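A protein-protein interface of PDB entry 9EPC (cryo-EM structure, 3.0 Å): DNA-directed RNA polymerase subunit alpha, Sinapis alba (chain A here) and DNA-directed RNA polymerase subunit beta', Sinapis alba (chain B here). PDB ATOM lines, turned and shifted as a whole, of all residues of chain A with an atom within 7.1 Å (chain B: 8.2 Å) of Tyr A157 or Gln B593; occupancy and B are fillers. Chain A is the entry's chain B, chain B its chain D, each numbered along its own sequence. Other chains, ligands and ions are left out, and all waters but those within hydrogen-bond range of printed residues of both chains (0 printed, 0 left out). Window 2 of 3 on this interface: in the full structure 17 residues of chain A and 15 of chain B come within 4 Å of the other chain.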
ATOM      1  N   ARG A  50       6.873 -23.618   3.129  1.00  0.00           N
ATOM      2  CA  ARG A  50       8.241 -24.064   3.366  1.00  0.00           C
ATOM      3  C   ARG A  50       8.785 -23.500   4.672  1.00  0.00           C
ATOM      4  O   ARG A  50       9.459 -24.208   5.427  1.00  0.00           O
ATOM      5  CB  ARG A  50       9.135 -23.670   2.192  1.00  0.00           C
ATOM      6  CG  ARG A  50      10.609 -23.904   2.448  1.00  0.00           C
ATOM      7  CD  ARG A  50      11.454 -23.608   1.225  1.00  0.00           C
ATOM      8  NE  ARG A  50      12.859 -23.454   1.579  1.00  0.00           N
ATOM      9  CZ  ARG A  50      13.705 -24.461   1.750  1.00  0.00           C
ATOM     10  NH1 ARG A  50      13.322 -25.717   1.599  1.00  0.00           N
ATOM     11  NH2 ARG A  50      14.965 -24.200   2.083  1.00  0.00           N
ATOM     12  N   ARG A  51       8.503 -22.227   4.957  1.00  0.00           N
ATOM     13  CA  ARG A  51       8.945 -21.646   6.220  1.00  0.00           C
ATOM     14  C   ARG A  51       8.274 -22.323   7.406  1.00  0.00           C
ATOM     15  O   ARG A  51       8.917 -22.581   8.429  1.00  0.00           O
ATOM     16  CB  ARG A  51       8.672 -20.144   6.240  1.00  0.00           C
ATOM     17  CG  ARG A  51       9.678 -19.324   5.465  1.00  0.00           C
ATOM     18  CD  ARG A  51       9.711 -17.900   5.973  1.00  0.00           C
ATOM     19  NE  ARG A  51       9.947 -17.851   7.411  1.00  0.00           N
ATOM     20  CZ  ARG A  51      11.147 -17.779   7.971  1.00  0.00           C
ATOM     21  NH1 ARG A  51      12.249 -17.743   7.242  1.00  0.00           N
ATOM     22  NH2 ARG A  51      11.242 -17.739   9.297  1.00  0.00           N
ATOM     23  N   ALA A  52       6.977 -22.609   7.293  1.00  0.00           N
ATOM     24  CA  ALA A  52       6.278 -23.283   8.380  1.00  0.00           C
ATOM     25  C   ALA A  52       6.818 -24.688   8.599  1.00  0.00           C
ATOM     26  O   ALA A  52       6.987 -25.122   9.743  1.00  0.00           O
ATOM     27  CB  ALA A  52       4.780 -23.324   8.095  1.00  0.00           C
ATOM     28  N   LEU A  53       7.088 -25.414   7.515  1.00  0.00           N
ATOM     29  CA  LEU A  53       7.561 -26.788   7.642  1.00  0.00           C
ATOM     30  C   LEU A  53       8.931 -26.850   8.302  1.00  0.00           C
ATOM     31  O   LEU A  53       9.190 -27.728   9.132  1.00  0.00           O
ATOM     32  CB  LEU A  53       7.599 -27.453   6.268  1.00  0.00           C
ATOM     33  CG  LEU A  53       6.248 -27.819   5.660  1.00  0.00           C
ATOM     34  CD1 LEU A  53       6.381 -28.023   4.167  1.00  0.00           C
ATOM     35  CD2 LEU A  53       5.706 -29.068   6.317  1.00  0.00           C
ATOM     36  N   LEU A  54       9.826 -25.929   7.945  1.00  0.00           N
ATOM     37  CA  LEU A  54      11.206 -26.035   8.404  1.00  0.00           C
ATOM     38  C   LEU A  54      11.347 -25.662   9.875  1.00  0.00           C
ATOM     39  O   LEU A  54      12.090 -26.316  10.614  1.00  0.00           O
ATOM     40  CB  LEU A  54      12.112 -25.162   7.540  1.00  0.00           C
ATOM     41  CG  LEU A  54      12.245 -25.606   6.083  1.00  0.00           C
ATOM     42  CD1 LEU A  54      13.205 -24.704   5.332  1.00  0.00           C
ATOM     43  CD2 LEU A  54      12.691 -27.052   6.003  1.00  0.00           C
ATOM     44  N   GLY A  55      10.655 -24.619  10.322  1.00  0.00           N
ATOM     45  CA  GLY A  55      10.866 -24.144  11.674  1.00  0.00           C
ATOM     46  C   GLY A  55       9.645 -24.058  12.566  1.00  0.00           C
ATOM     47  O   GLY A  55       9.772 -24.127  13.791  1.00  0.00           O
ATOM     48  N   GLU A  56       8.460 -23.909  11.982  1.00  0.00           N
ATOM     49  CA  GLU A  56       7.261 -23.677  12.777  1.00  0.00           C
ATOM     50  C   GLU A  56       6.625 -24.956  13.300  1.00  0.00           C
ATOM     51  O   GLU A  56       5.642 -24.876  14.043  1.00  0.00           O
ATOM     52  CB  GLU A  56       6.228 -22.898  11.965  1.00  0.00           C
ATOM     53  CG  GLU A  56       6.686 -21.523  11.523  1.00  0.00           C
ATOM     54  CD  GLU A  56       6.725 -20.525  12.657  1.00  0.00           C
ATOM     55  OE1 GLU A  56       6.206 -20.837  13.750  1.00  0.00           O
ATOM     56  OE2 GLU A  56       7.275 -19.423  12.456  1.00  0.00           O
ATOM     57  N   ILE A  57       7.145 -26.121  12.939  1.00  0.00           N
ATOM     58  CA  ILE A  57       6.581 -27.388  13.384  1.00  0.00           C
ATOM     59  C   ILE A  57       7.301 -27.826  14.649  1.00  0.00           C
ATOM     60  O   ILE A  57       8.536 -27.832  14.702  1.00  0.00           O
ATOM     61  CB  ILE A  57       6.688 -28.457  12.286  1.00  0.00           C
ATOM     62  CG1 ILE A  57       5.889 -28.027  11.059  1.00  0.00           C
ATOM     63  CG2 ILE A  57       6.185 -29.791  12.794  1.00  0.00           C
ATOM     64  CD1 ILE A  57       5.787 -29.094  10.002  1.00  0.00           C
ATOM     65  N   ASN A 154      10.197 -28.106  21.273  1.00  0.00           N
ATOM     66  CA  ASN A 154      10.208 -26.719  20.835  1.00  0.00           C
ATOM     67  C   ASN A 154      10.102 -26.670  19.317  1.00  0.00           C
ATOM     68  O   ASN A 154      10.099 -27.698  18.636  1.00  0.00           O
ATOM     69  CB  ASN A 154      11.475 -25.992  21.302  1.00  0.00           C
ATOM     70  CG  ASN A 154      11.682 -26.086  22.794  1.00  0.00           C
ATOM     71  OD1 ASN A 154      12.759 -26.455  23.258  1.00  0.00           O
ATOM     72  ND2 ASN A 154      10.651 -25.749  23.557  1.00  0.00           N
ATOM     73  N   ARG A 155      10.009 -25.456  18.789  1.00  0.00           N
ATOM     74  CA  ARG A 155      10.016 -25.232  17.355  1.00  0.00           C
ATOM     75  C   ARG A 155      11.446 -25.143  16.841  1.00  0.00           C
ATOM     76  O   ARG A 155      12.398 -24.961  17.602  1.00  0.00           O
ATOM     77  CB  ARG A 155       9.258 -23.956  17.001  1.00  0.00           C
ATOM     78  CG  ARG A 155       7.833 -23.922  17.496  1.00  0.00           C
ATOM     79  CD  ARG A 155       7.200 -22.578  17.209  1.00  0.00           C
ATOM     80  NE  ARG A 155       8.103 -21.479  17.523  1.00  0.00           N
ATOM     81  CZ  ARG A 155       8.579 -20.621  16.633  1.00  0.00           C
ATOM     82  NH1 ARG A 155       8.228 -20.679  15.361  1.00  0.00           N
ATOM     83  NH2 ARG A 155       9.424 -19.676  17.031  1.00  0.00           N
ATOM     84  N   GLY A 156      11.588 -25.278  15.523  1.00  0.00           N
ATOM     85  CA  GLY A 156      12.907 -25.185  14.923  1.00  0.00           C
ATOM     86  C   GLY A 156      13.513 -23.802  15.047  1.00  0.00           C
ATOM     87  O   GLY A 156      14.706 -23.662  15.329  1.00  0.00           O
ATOM     88  N   TYR A 157      12.705 -22.764  14.841  1.00  0.00           N
ATOM     89  CA  TYR A 157      13.210 -21.398  14.855  1.00  0.00           C
ATOM     90  C   TYR A 157      13.465 -20.866  16.257  1.00  0.00           C
ATOM     91  O   TYR A 157      14.193 -19.881  16.406  1.00  0.00           O
ATOM     92  CB  TYR A 157      12.230 -20.474  14.134  1.00  0.00           C
ATOM     93  CG  TYR A 157      12.130 -20.727  12.650  1.00  0.00           C
ATOM     94  CD1 TYR A 157      13.238 -21.129  11.921  1.00  0.00           C
ATOM     95  CD2 TYR A 157      10.928 -20.565  11.980  1.00  0.00           C
ATOM     96  CE1 TYR A 157      13.151 -21.359  10.565  1.00  0.00           C
ATOM     97  CE2 TYR A 157      10.832 -20.793  10.624  1.00  0.00           C
ATOM     98  CZ  TYR A 157      11.946 -21.191   9.923  1.00  0.00           C
ATOM     99  OH  TYR A 157      11.853 -21.420   8.571  1.00  0.00           O
ATOM    100  N   SER A 158      12.890 -21.489  17.281  1.00  0.00           N
ATOM    101  CA  SER A 158      13.032 -20.980  18.634  1.00  0.00           C
ATOM    102  C   SER A 158      14.450 -21.198  19.151  1.00  0.00           C
ATOM    103  O   SER A 158      15.179 -22.087  18.704  1.00  0.00           O
ATOM    104  CB  SER A 158      12.030 -21.655  19.567  1.00  0.00           C
ATOM    105  OG  SER A 158      12.301 -23.039  19.684  1.00  0.00           O
ATOM    106  N   LEU A 159      14.838 -20.363  20.112  1.00  0.00           N
ATOM    107  CA  LEU A 159      16.127 -20.468  20.777  1.00  0.00           C
ATOM    108  C   LEU A 159      15.917 -20.503  22.283  1.00  0.00           C
ATOM    109  O   LEU A 159      15.012 -19.847  22.806  1.00  0.00           O
ATOM    110  CB  LEU A 159      17.050 -19.300  20.413  1.00  0.00           C
ATOM    111  CG  LEU A 159      17.520 -19.209  18.962  1.00  0.00           C
ATOM    112  CD1 LEU A 159      18.523 -18.081  18.803  1.00  0.00           C
ATOM    113  CD2 LEU A 159      18.117 -20.530  18.508  1.00  0.00           C
ATOM    114  N   ALA A 174      20.667 -29.845  20.357  1.00  0.00           N
ATOM    115  CA  ALA A 174      19.693 -30.578  19.563  1.00  0.00           C
ATOM    116  C   ALA A 174      18.994 -29.643  18.589  1.00  0.00           C
ATOM    117  O   ALA A 174      18.493 -28.586  18.983  1.00  0.00           O
ATOM    118  CB  ALA A 174      18.670 -31.258  20.470  1.00  0.00           C
ATOM    119  N   VAL A 175      18.965 -30.035  17.322  1.00  0.00           N
ATOM    120  CA  VAL A 175      18.209 -29.323  16.301  1.00  0.00           C
ATOM    121  C   VAL A 175      16.789 -29.866  16.299  1.00  0.00           C
ATOM    122  O   VAL A 175      16.581 -31.084  16.258  1.00  0.00           O
ATOM    123  CB  VAL A 175      18.865 -29.477  14.921  1.00  0.00           C
ATOM    124  CG1 VAL A 175      18.143 -28.624  13.898  1.00  0.00           C
ATOM    125  CG2 VAL A 175      20.332 -29.099  14.991  1.00  0.00           C
ATOM    126  N   PHE A 176      15.811 -28.966  16.337  1.00  0.00           N
ATOM    127  CA  PHE A 176      14.410 -29.332  16.531  1.00  0.00           C
ATOM    128  C   PHE A 176      13.647 -29.417  15.220  1.00  0.00           C
ATOM    129  O   PHE A 176      12.479 -29.026  15.156  1.00  0.00           O
ATOM    130  CB  PHE A 176      13.733 -28.344  17.473  1.00  0.00           C
ATOM    131  CG  PHE A 176      14.089 -28.538  18.913  1.00  0.00           C
ATOM    132  CD1 PHE A 176      15.227 -27.965  19.442  1.00  0.00           C
ATOM    133  CD2 PHE A 176      13.277 -29.287  19.742  1.00  0.00           C
ATOM    134  CE1 PHE A 176      15.552 -28.142  20.767  1.00  0.00           C
ATOM    135  CE2 PHE A 176      13.597 -29.465  21.069  1.00  0.00           C
ATOM    136  CZ  PHE A 176      14.736 -28.894  21.581  1.00  0.00           C
ATOM    137  N   MET A 177      14.270 -29.910  14.153  1.00  0.00           N
ATOM    138  CA  MET A 177      13.567 -30.023  12.886  1.00  0.00           C
ATOM    139  C   MET A 177      13.010 -31.429  12.726  1.00  0.00           C
ATOM    140  O   MET A 177      13.789 -32.392  12.659  1.00  0.00           O
ATOM    141  CB  MET A 177      14.486 -29.673  11.716  1.00  0.00           C
ATOM    142  CG  MET A 177      15.834 -30.366  11.716  1.00  0.00           C
ATOM    143  SD  MET A 177      16.816 -29.907  10.280  1.00  0.00           S
ATOM    144  CE  MET A 177      18.048 -31.202  10.282  1.00  0.00           C
ATOM    145  N   PRO A 178      11.694 -31.605  12.689  1.00  0.00           N
ATOM    146  CA  PRO A 178      11.136 -32.922  12.373  1.00  0.00           C
ATOM    147  C   PRO A 178      10.974 -33.107  10.875  1.00  0.00           C
ATOM    148  O   PRO A 178      10.837 -34.232  10.386  1.00  0.00           O
ATOM    149  CB  PRO A 178       9.786 -32.905  13.093  1.00  0.00           C
ATOM    150  CG  PRO A 178       9.386 -31.477  13.046  1.00  0.00           C
ATOM    151  CD  PRO A 178      10.651 -30.659  13.122  1.00  0.00           C
ATOM    152  N   VAL A 179      10.983 -32.003  10.140  1.00  0.00           N
ATOM    153  CA  VAL A 179      10.907 -32.015   8.687  1.00  0.00           C
ATOM    154  C   VAL A 179      12.326 -31.799   8.180  1.00  0.00           C
ATOM    155  O   VAL A 179      12.863 -30.692   8.254  1.00  0.00           O
ATOM    156  CB  VAL A 179       9.942 -30.951   8.159  1.00  0.00           C
ATOM    157  CG1 VAL A 179       9.980 -30.906   6.647  1.00  0.00           C
ATOM    158  CG2 VAL A 179       8.537 -31.237   8.646  1.00  0.00           C
ATOM    159  N   ASP B 586      22.077 -32.272   9.522  1.00  0.00           N
ATOM    160  CA  ASP B 586      21.805 -31.358  10.626  1.00  0.00           C
ATOM    161  C   ASP B 586      22.503 -30.021  10.421  1.00  0.00           C
ATOM    162  O   ASP B 586      21.938 -28.968  10.735  1.00  0.00           O
ATOM    163  CB  ASP B 586      22.230 -31.986  11.950  1.00  0.00           C
ATOM    164  CG  ASP B 586      21.357 -33.155  12.341  1.00  0.00           C
ATOM    165  OD1 ASP B 586      20.542 -33.592  11.504  1.00  0.00           O
ATOM    166  OD2 ASP B 586      21.481 -33.635  13.486  1.00  0.00           O
ATOM    167  N   ALA B 587      23.732 -30.043   9.902  1.00  0.00           N
ATOM    168  CA  ALA B 587      24.438 -28.796   9.633  1.00  0.00           C
ATOM    169  C   ALA B 587      23.696 -27.959   8.602  1.00  0.00           C
ATOM    170  O   ALA B 587      23.567 -26.740   8.757  1.00  0.00           O
ATOM    171  CB  ALA B 587      25.862 -29.087   9.166  1.00  0.00           C
ATOM    172  N   ILE B 588      23.203 -28.596   7.539  1.00  0.00           N
ATOM    173  CA  ILE B 588      22.398 -27.879   6.554  1.00  0.00           C
ATOM    174  C   ILE B 588      21.100 -27.395   7.182  1.00  0.00           C
ATOM    175  O   ILE B 588      20.682 -26.250   6.978  1.00  0.00           O
ATOM    176  CB  ILE B 588      22.132 -28.770   5.328  1.00  0.00           C
ATOM    177  CG1 ILE B 588      23.447 -29.162   4.658  1.00  0.00           C
ATOM    178  CG2 ILE B 588      21.228 -28.056   4.343  1.00  0.00           C
ATOM    179  CD1 ILE B 588      24.229 -27.992   4.134  1.00  0.00           C
ATOM    180  N   GLY B 589      20.444 -28.258   7.958  1.00  0.00           N
ATOM    181  CA  GLY B 589      19.187 -27.876   8.577  1.00  0.00           C
ATOM    182  C   GLY B 589      19.341 -26.731   9.558  1.00  0.00           C
ATOM    183  O   GLY B 589      18.506 -25.824   9.604  1.00  0.00           O
ATOM    184  N   ALA B 590      20.407 -26.756  10.358  1.00  0.00           N
ATOM    185  CA  ALA B 590      20.661 -25.656  11.281  1.00  0.00           C
ATOM    186  C   ALA B 590      20.906 -24.357  10.526  1.00  0.00           C
ATOM    187  O   ALA B 590      20.490 -23.282  10.972  1.00  0.00           O
ATOM    188  CB  ALA B 590      21.849 -25.985  12.180  1.00  0.00           C
ATOM    189  N   TYR B 591      21.584 -24.438   9.380  1.00  0.00           N
ATOM    190  CA  TYR B 591      21.803 -23.249   8.565  1.00  0.00           C
ATOM    191  C   TYR B 591      20.488 -22.693   8.036  1.00  0.00           C
ATOM    192  O   TYR B 591      20.303 -21.473   7.974  1.00  0.00           O
ATOM    193  CB  TYR B 591      22.750 -23.571   7.414  1.00  0.00           C
ATOM    194  CG  TYR B 591      22.834 -22.486   6.372  1.00  0.00           C
ATOM    195  CD1 TYR B 591      23.401 -21.258   6.666  1.00  0.00           C
ATOM    196  CD2 TYR B 591      22.352 -22.694   5.089  1.00  0.00           C
ATOM    197  CE1 TYR B 591      23.482 -20.266   5.716  1.00  0.00           C
ATOM    198  CE2 TYR B 591      22.428 -21.708   4.133  1.00  0.00           C
ATOM    199  CZ  TYR B 591      22.994 -20.495   4.452  1.00  0.00           C
ATOM    200  OH  TYR B 591      23.074 -19.507   3.500  1.00  0.00           O
ATOM    201  N   ARG B 592      19.565 -23.572   7.641  1.00  0.00           N
ATOM    202  CA  ARG B 592      18.261 -23.112   7.180  1.00  0.00           C
ATOM    203  C   ARG B 592      17.506 -22.401   8.294  1.00  0.00           C
ATOM    204  O   ARG B 592      16.836 -21.391   8.054  1.00  0.00           O
ATOM    205  CB  ARG B 592      17.445 -24.288   6.649  1.00  0.00           C
ATOM    206  CG  ARG B 592      18.021 -24.924   5.404  1.00  0.00           C
ATOM    207  CD  ARG B 592      17.311 -26.221   5.078  1.00  0.00           C
ATOM    208  NE  ARG B 592      17.952 -26.923   3.975  1.00  0.00           N
ATOM    209  CZ  ARG B 592      17.680 -28.173   3.624  1.00  0.00           C
ATOM    210  NH1 ARG B 592      16.780 -28.891   4.276  1.00  0.00           N
ATOM    211  NH2 ARG B 592      18.328 -28.716   2.599  1.00  0.00           N
ATOM    212  N   GLN B 593      17.604 -22.911   9.517  1.00  0.00           N
ATOM    213  CA  GLN B 593      16.942 -22.313  10.666  1.00  0.00           C
ATOM    214  C   GLN B 593      17.692 -21.113  11.224  1.00  0.00           C
ATOM    215  O   GLN B 593      17.414 -20.697  12.354  1.00  0.00           O
ATOM    216  CB  GLN B 593      16.744 -23.362  11.759  1.00  0.00           C
ATOM    217  CG  GLN B 593      15.944 -24.562  11.304  1.00  0.00           C
ATOM    218  CD  GLN B 593      15.697 -25.548  12.420  1.00  0.00           C
ATOM    219  OE1 GLN B 593      16.344 -25.495  13.463  1.00  0.00           O
ATOM    220  NE2 GLN B 593      14.750 -26.450  12.210  1.00  0.00           N
ATOM    221  N   LYS B 594      18.643 -20.566  10.466  1.00  0.00           N
ATOM    222  CA  LYS B 594      19.392 -19.367  10.834  1.00  0.00           C
ATOM    223  C   LYS B 594      20.178 -19.544  12.128  1.00  0.00           C
ATOM    224  O   LYS B 594      20.576 -18.559  12.754  1.00  0.00           O
ATOM    225  CB  LYS B 594      18.470 -18.148  10.944  1.00  0.00           C
ATOM    226  CG  LYS B 594      17.651 -17.879   9.696  1.00  0.00           C
ATOM    227  CD  LYS B 594      18.543 -17.643   8.492  1.00  0.00           C
ATOM    228  CE  LYS B 594      17.722 -17.345   7.250  1.00  0.00           C
ATOM    229  NZ  LYS B 594      18.583 -17.071   6.067  1.00  0.00           N
ATOM    230  N   ARG B 595      20.414 -20.788  12.544  1.00  0.00           N
ATOM    231  CA  ARG B 595      21.163 -21.015  13.773  1.00  0.00           C
ATOM    232  C   ARG B 595      22.643 -20.712  13.591  1.00  0.00           C
ATOM    233  O   ARG B 595      23.296 -20.235  14.524  1.00  0.00           O
ATOM    234  CB  ARG B 595      20.962 -22.451  14.251  1.00  0.00           C
ATOM    235  CG  ARG B 595      21.634 -22.760  15.574  1.00  0.00           C
ATOM    236  CD  ARG B 595      21.158 -24.086  16.131  1.00  0.00           C
ATOM    237  NE  ARG B 595      19.709 -24.117  16.277  1.00  0.00           N
ATOM    238  CZ  ARG B 595      19.035 -25.106  16.846  1.00  0.00           C
ATOM    239  NH1 ARG B 595      19.653 -26.162  17.349  1.00  0.00           N
ATOM    240  NH2 ARG B 595      17.710 -25.033  16.914  1.00  0.00           N
ATOM    241  N   ILE B 596      23.190 -20.982  12.406  1.00  0.00           N
ATOM    242  CA  ILE B 596      24.588 -20.710  12.109  1.00  0.00           C
ATOM    243  C   ILE B 596      24.676 -20.007  10.764  1.00  0.00           C
ATOM    244  O   ILE B 596      23.797 -20.133   9.909  1.00  0.00           O
ATOM    245  CB  ILE B 596      25.443 -21.992  12.098  1.00  0.00           C
ATOM    246  CG1 ILE B 596      24.844 -23.013  11.135  1.00  0.00           C
ATOM    247  CG2 ILE B 596      25.553 -22.573  13.496  1.00  0.00           C
ATOM    248  CD1 ILE B 596      25.560 -24.333  11.135  1.00  0.00           C
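Hydrophobic or aromatic side chains of chain A within 4 Å of the printed part of chain B: Tyr A157, Val A175 and Met A177. Among the printed residues, no Asp or Glu carboxylate lies within 4 Å of a Lys or Arg side-chain nitrogen of the other chain.
The side-chain hydroxyl (OH) of Tyr A157 lies within hydrogen-bond range of the backbone carbonyl oxygen (O) of Arg A51 (3.2 Å). The backbone carbonyl oxygen of Gly A55 lies within hydrogen-bond range of the backbone NH of Tyr A157 (3.4 Å). The backbone NH of Gly A156 lies within hydrogen-bond range of the backbone carbonyl oxygen of Gly A55 (2.8 Å). The backbone carbonyl oxygen of Ala B590 sits at hydrogen-bond distance from the backbone NH of Arg B595.
O of Leu A54 lies within hydrogen-bond range of NE2 of Gln B593 (3.1 Å). NH1 of Arg B595 lies within hydrogen-bond range of O of Ala A174 (3.1 Å). O of Gly A156 sits close to OE1 of Gln B593 (3.1 Å).
Gly A156 touches Arg B595. CA of Gln B593 touches CE1 of Tyr A157, 3.9 Å away. CG1 of Val A175 touches OE1 of Gln B593, at 3.6 Å. Val A175 touches Arg B595 (CA to NH1, 3.6 Å). OD1 of Asp B586 touches CE of Met A177, 3.7 Å away. Met A177 touches Gly B589. Gln B593 touches Met A177.
Tyr A157 touches just one residue of chain B: Gln B593 (3.9 Å). Of chain A, only Leu A54, Gly A156, Tyr A157, Val A175 and Met A177 come within 4 Å of Gln B593. Gly A156 touches two residues of chain B. Of the printed residues of chain B, Met A177 touches Asp B586 (3.7 Å), Gly B589 (3.6 Å) and Gln B593 (3.3 Å). Printed residues of chain A within 4 Å of Arg B595: Gly A156, Ala A174 and Val A175. Printed residues of chain B within 4 Å of Leu A54: Gln B593 (3.1 Å). Of the printed residues of chain A, Asp B586 touches Met A177. Of the printed residues of chain B, Val A175 touches Gln B593 (3.6 Å) and Arg B595 (3.6 Å). Ala B587 touches none of the printed residues of chain A. The nearest residue of chain A that does not touch Gln B593 is Phe A176 (4.4 Å).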
